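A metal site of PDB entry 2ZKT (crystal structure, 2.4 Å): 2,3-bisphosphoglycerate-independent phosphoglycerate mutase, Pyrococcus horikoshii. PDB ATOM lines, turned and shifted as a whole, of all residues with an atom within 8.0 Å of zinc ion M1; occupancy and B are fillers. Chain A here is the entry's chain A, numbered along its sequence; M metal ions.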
ATOM      1  N   ASP A  13     -16.547  13.724  24.488  1.00  0.00           N
ATOM      2  CA  ASP A  13     -15.252  13.057  24.630  1.00  0.00           C
ATOM      3  C   ASP A  13     -14.075  14.007  24.369  1.00  0.00           C
ATOM      4  O   ASP A  13     -14.068  14.753  23.394  1.00  0.00           O
ATOM      5  CB  ASP A  13     -15.212  11.849  23.675  1.00  0.00           C
ATOM      6  CG  ASP A  13     -14.434  10.676  24.261  1.00  0.00           C
ATOM      7  OD1 ASP A  13     -13.179  10.759  24.305  1.00  0.00           O
ATOM      8  OD2 ASP A  13     -15.072   9.672  24.682  1.00  0.00           O
ATOM      9  N   GLY A  14     -13.088  13.970  25.274  1.00  0.00           N
ATOM     10  CA  GLY A  14     -11.899  14.815  25.138  1.00  0.00           C
ATOM     11  C   GLY A  14     -12.074  16.347  25.136  1.00  0.00           C
ATOM     12  O   GLY A  14     -11.151  17.068  24.726  1.00  0.00           O
ATOM     13  N   ALA A  58      -6.699   9.580  32.085  1.00  0.00           N
ATOM     14  CA  ALA A  58      -7.543   8.387  32.141  1.00  0.00           C
ATOM     15  C   ALA A  58      -8.005   7.958  30.757  1.00  0.00           C
ATOM     16  O   ALA A  58      -8.316   8.802  29.902  1.00  0.00           O
ATOM     17  CB  ALA A  58      -8.756   8.640  33.031  1.00  0.00           C
ATOM     18  N   GLY A  59      -8.057   6.642  30.528  1.00  0.00           N
ATOM     19  CA  GLY A  59      -8.534   6.140  29.249  1.00  0.00           C
ATOM     20  C   GLY A  59     -10.032   6.387  29.160  1.00  0.00           C
ATOM     21  O   GLY A  59     -10.683   6.676  30.176  1.00  0.00           O
ATOM     22  N   SER A  60     -10.595   6.271  27.955  1.00  0.00           N
ATOM     23  CA  SER A  60     -12.036   6.508  27.779  1.00  0.00           C
ATOM     24  C   SER A  60     -12.898   5.584  28.658  1.00  0.00           C
ATOM     25  O   SER A  60     -13.963   5.976  29.139  1.00  0.00           O
ATOM     26  CB  SER A  60     -12.401   6.330  26.302  1.00  0.00           C
ATOM     27  OG  SER A  60     -13.476   7.196  25.955  1.00  0.00           O
ATOM     28  N   LEU A 254     -16.577   0.961  22.745  1.00  0.00           N
ATOM     29  CA  LEU A 254     -15.983   1.028  24.074  1.00  0.00           C
ATOM     30  C   LEU A 254     -16.881   1.641  25.151  1.00  0.00           C
ATOM     31  O   LEU A 254     -17.033   1.071  26.240  1.00  0.00           O
ATOM     32  CB  LEU A 254     -14.657   1.806  24.019  1.00  0.00           C
ATOM     33  CG  LEU A 254     -13.878   1.837  25.343  1.00  0.00           C
ATOM     34  CD1 LEU A 254     -13.930   0.454  26.011  1.00  0.00           C
ATOM     35  CD2 LEU A 254     -12.444   2.269  25.076  1.00  0.00           C
ATOM     36  N   LYS A 302     -18.423  11.309  20.514  1.00  0.00           N
ATOM     37  CA  LYS A 302     -17.016  10.930  20.321  1.00  0.00           C
ATOM     38  C   LYS A 302     -16.053  11.858  19.564  1.00  0.00           C
ATOM     39  O   LYS A 302     -14.983  12.200  20.072  1.00  0.00           O
ATOM     40  CB  LYS A 302     -16.960   9.533  19.682  1.00  0.00           C
ATOM     41  CG  LYS A 302     -15.563   8.906  19.674  1.00  0.00           C
ATOM     42  CD  LYS A 302     -15.043   8.746  21.091  1.00  0.00           C
ATOM     43  CE  LYS A 302     -13.637   8.189  21.098  1.00  0.00           C
ATOM     44  NZ  LYS A 302     -12.767   8.960  20.173  1.00  0.00           N
ATOM     45  N   THR A 304     -15.166  14.943  19.085  1.00  0.00           N
ATOM     46  CA  THR A 304     -14.307  15.974  19.674  1.00  0.00           C
ATOM     47  C   THR A 304     -12.947  15.364  20.044  1.00  0.00           C
ATOM     48  O   THR A 304     -11.895  15.956  19.795  1.00  0.00           O
ATOM     49  CB  THR A 304     -14.926  16.622  20.943  1.00  0.00           C
ATOM     50  OG1 THR A 304     -15.504  15.607  21.770  1.00  0.00           O
ATOM     51  CG2 THR A 304     -16.009  17.626  20.564  1.00  0.00           C
ATOM     52  N   ASP A 305     -12.984  14.167  20.624  1.00  0.00           N
ATOM     53  CA  ASP A 305     -11.745  13.496  21.030  1.00  0.00           C
ATOM     54  C   ASP A 305     -10.816  13.139  19.873  1.00  0.00           C
ATOM     55  O   ASP A 305      -9.588  13.229  20.009  1.00  0.00           O
ATOM     56  CB  ASP A 305     -12.091  12.231  21.830  1.00  0.00           C
ATOM     57  CG  ASP A 305     -10.857  11.456  22.278  1.00  0.00           C
ATOM     58  OD1 ASP A 305      -9.969  12.050  22.952  1.00  0.00           O
ATOM     59  OD2 ASP A 305     -10.781  10.250  21.968  1.00  0.00           O
ATOM     60  N   ALA A 306     -11.384  12.746  18.735  1.00  0.00           N
ATOM     61  CA  ALA A 306     -10.582  12.376  17.568  1.00  0.00           C
ATOM     62  C   ALA A 306      -9.736  13.557  17.105  1.00  0.00           C
ATOM     63  O   ALA A 306      -8.538  13.400  16.846  1.00  0.00           O
ATOM     64  CB  ALA A 306     -11.487  11.896  16.428  1.00  0.00           C
ATOM     65  N   GLY A 308      -8.708  15.992  18.811  1.00  0.00           N
ATOM     66  CA  GLY A 308      -7.655  16.255  19.783  1.00  0.00           C
ATOM     67  C   GLY A 308      -6.446  15.387  19.503  1.00  0.00           C
ATOM     68  O   GLY A 308      -5.312  15.873  19.559  1.00  0.00           O
ATOM     69  N   HIS A 309      -6.680  14.110  19.190  1.00  0.00           N
ATOM     70  CA  HIS A 309      -5.587  13.174  18.889  1.00  0.00           C
ATOM     71  C   HIS A 309      -4.763  13.594  17.677  1.00  0.00           C
ATOM     72  O   HIS A 309      -3.525  13.460  17.685  1.00  0.00           O
ATOM     73  CB  HIS A 309      -6.147  11.763  18.644  1.00  0.00           C
ATOM     74  CG  HIS A 309      -6.477  11.011  19.906  1.00  0.00           C
ATOM     75  ND1 HIS A 309      -5.506  10.502  20.754  1.00  0.00           N
ATOM     76  CD2 HIS A 309      -7.668  10.669  20.454  1.00  0.00           C
ATOM     77  CE1 HIS A 309      -6.079   9.897  21.777  1.00  0.00           C
ATOM     78  NE2 HIS A 309      -7.394   9.979  21.621  1.00  0.00           N
ATOM     79  N   ASP A 346     -15.075  13.368  29.483  1.00  0.00           N
ATOM     80  CA  ASP A 346     -14.568  12.304  30.356  1.00  0.00           C
ATOM     81  C   ASP A 346     -13.069  12.480  30.650  1.00  0.00           C
ATOM     82  O   ASP A 346     -12.497  11.827  31.509  1.00  0.00           O
ATOM     83  CB  ASP A 346     -14.835  10.952  29.682  1.00  0.00           C
ATOM     84  CG  ASP A 346     -14.235  10.949  28.276  1.00  0.00           C
ATOM     85  OD1 ASP A 346     -14.250  12.011  27.638  1.00  0.00           O
ATOM     86  OD2 ASP A 346     -13.748   9.904  27.840  1.00  0.00           O
ATOM     87  N   HIS A 347     -12.427  13.367  29.857  1.00  0.00           N
ATOM     88  CA  HIS A 347     -11.034  13.699  30.126  1.00  0.00           C
ATOM     89  C   HIS A 347     -10.525  14.814  29.184  1.00  0.00           C
ATOM     90  O   HIS A 347     -11.232  15.302  28.312  1.00  0.00           O
ATOM     91  CB  HIS A 347     -10.176  12.433  29.937  1.00  0.00           C
ATOM     92  CG  HIS A 347     -10.421  11.863  28.570  1.00  0.00           C
ATOM     93  ND1 HIS A 347      -9.965  12.439  27.424  1.00  0.00           N
ATOM     94  CD2 HIS A 347     -11.094  10.679  28.231  1.00  0.00           C
ATOM     95  CE1 HIS A 347     -10.345  11.630  26.419  1.00  0.00           C
ATOM     96  NE2 HIS A 347     -11.031  10.565  26.870  1.00  0.00           N
ATOM     97  N   SER A 348      -9.274  15.257  29.342  1.00  0.00           N
ATOM     98  CA  SER A 348      -8.739  16.289  28.460  1.00  0.00           C
ATOM     99  C   SER A 348      -7.888  15.605  27.415  1.00  0.00           C
ATOM    100  O   SER A 348      -7.157  14.660  27.721  1.00  0.00           O
ATOM    101  CB  SER A 348      -7.861  17.280  29.236  1.00  0.00           C
ATOM    102  OG  SER A 348      -8.656  18.120  30.056  1.00  0.00           O
ATOM    103  N   THR A 349      -8.011  16.067  26.167  1.00  0.00           N
ATOM    104  CA  THR A 349      -7.222  15.553  25.053  1.00  0.00           C
ATOM    105  C   THR A 349      -6.736  16.808  24.347  1.00  0.00           C
ATOM    106  O   THR A 349      -7.313  17.249  23.340  1.00  0.00           O
ATOM    107  CB  THR A 349      -8.067  14.721  24.072  1.00  0.00           C
ATOM    108  OG1 THR A 349      -8.641  13.605  24.760  1.00  0.00           O
ATOM    109  CG2 THR A 349      -7.188  14.199  22.925  1.00  0.00           C
ATOM    110  N   MET A 354      -1.868  15.456  21.599  1.00  0.00           N
ATOM    111  CA  MET A 354      -2.308  14.385  20.702  1.00  0.00           C
ATOM    112  C   MET A 354      -2.600  13.103  21.491  1.00  0.00           C
ATOM    113  O   MET A 354      -2.451  11.992  20.987  1.00  0.00           O
ATOM    114  CB  MET A 354      -1.230  14.134  19.632  1.00  0.00           C
ATOM    115  CG  MET A 354      -0.860  15.414  18.860  1.00  0.00           C
ATOM    116  SD  MET A 354       0.417  15.193  17.599  1.00  0.00           S
ATOM    117  CE  MET A 354      -0.612  14.691  16.169  1.00  0.00           C
ATOM    118  N   ASN A 355      -3.015  13.286  22.747  1.00  0.00           N
ATOM    119  CA  ASN A 355      -3.349  12.179  23.631  1.00  0.00           C
ATOM    120  C   ASN A 355      -4.010  12.728  24.912  1.00  0.00           C
ATOM    121  O   ASN A 355      -4.046  13.934  25.144  1.00  0.00           O
ATOM    122  CB  ASN A 355      -2.096  11.394  24.009  1.00  0.00           C
ATOM    123  CG  ASN A 355      -2.353   9.893  24.050  1.00  0.00           C
ATOM    124  OD1 ASN A 355      -3.352   9.437  24.612  1.00  0.00           O
ATOM    125  ND2 ASN A 355      -1.446   9.125  23.450  1.00  0.00           N
ATOM    126  N   HIS A 356      -4.526  11.817  25.735  1.00  0.00           N
ATOM    127  CA  HIS A 356      -5.192  12.210  26.969  1.00  0.00           C
ATOM    128  C   HIS A 356      -4.211  12.832  27.959  1.00  0.00           C
ATOM    129  O   HIS A 356      -3.091  12.334  28.147  1.00  0.00           O
ATOM    130  CB  HIS A 356      -5.874  10.986  27.606  1.00  0.00           C
ATOM    131  CG  HIS A 356      -6.856  10.298  26.705  1.00  0.00           C
ATOM    132  ND1 HIS A 356      -7.633   9.230  27.124  1.00  0.00           N
ATOM    133  CD2 HIS A 356      -7.192  10.517  25.408  1.00  0.00           C
ATOM    134  CE1 HIS A 356      -8.400   8.821  26.126  1.00  0.00           C
ATOM    135  NE2 HIS A 356      -8.157   9.598  25.070  1.00  0.00           N
HETATM  136 ZN    ZN M   1      -9.145   9.186  22.980  1.00  0.00          ZN
HETATM  137 ZN    ZN M   2     -12.694   9.224  25.934  1.00  0.00          ZN
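OD2 of Asp 305 sits close to NZ of Lys 302. The backbone NH (N) of Asp 305 lies within hydrogen-bond range of the backbone carbonyl oxygen (O) of Asp 13, at 3.0 Å. A ring nitrogen (ND1) of His 309 sits at hydrogen-bond distance from the backbone carbonyl oxygen of Met 354 (3.4 Å). The side-chain carboxylate (OD1) of Asp 305 sits at hydrogen-bond distance from the side-chain hydroxyl (OG1) of Thr 349, 2.7 Å away. A ring nitrogen (ND1) of His 356 is in hydrogen-bond range of the backbone carbonyl oxygen of Ala 58 (2.9 Å).
Within 4 Å of zinc ion M1: Asp 305, His 309 and His 356. The nearest printed residue that does not touch zinc ion M1 is His 347 (4.4 Å).
Zinc ion M1 is bound by the side-chain carboxylate of Asp 305 (2.2 Å), a ring nitrogen (NE2) of His 356 (2.3 Å) and a ring nitrogen (NE2) of His 309 (2.4 Å).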
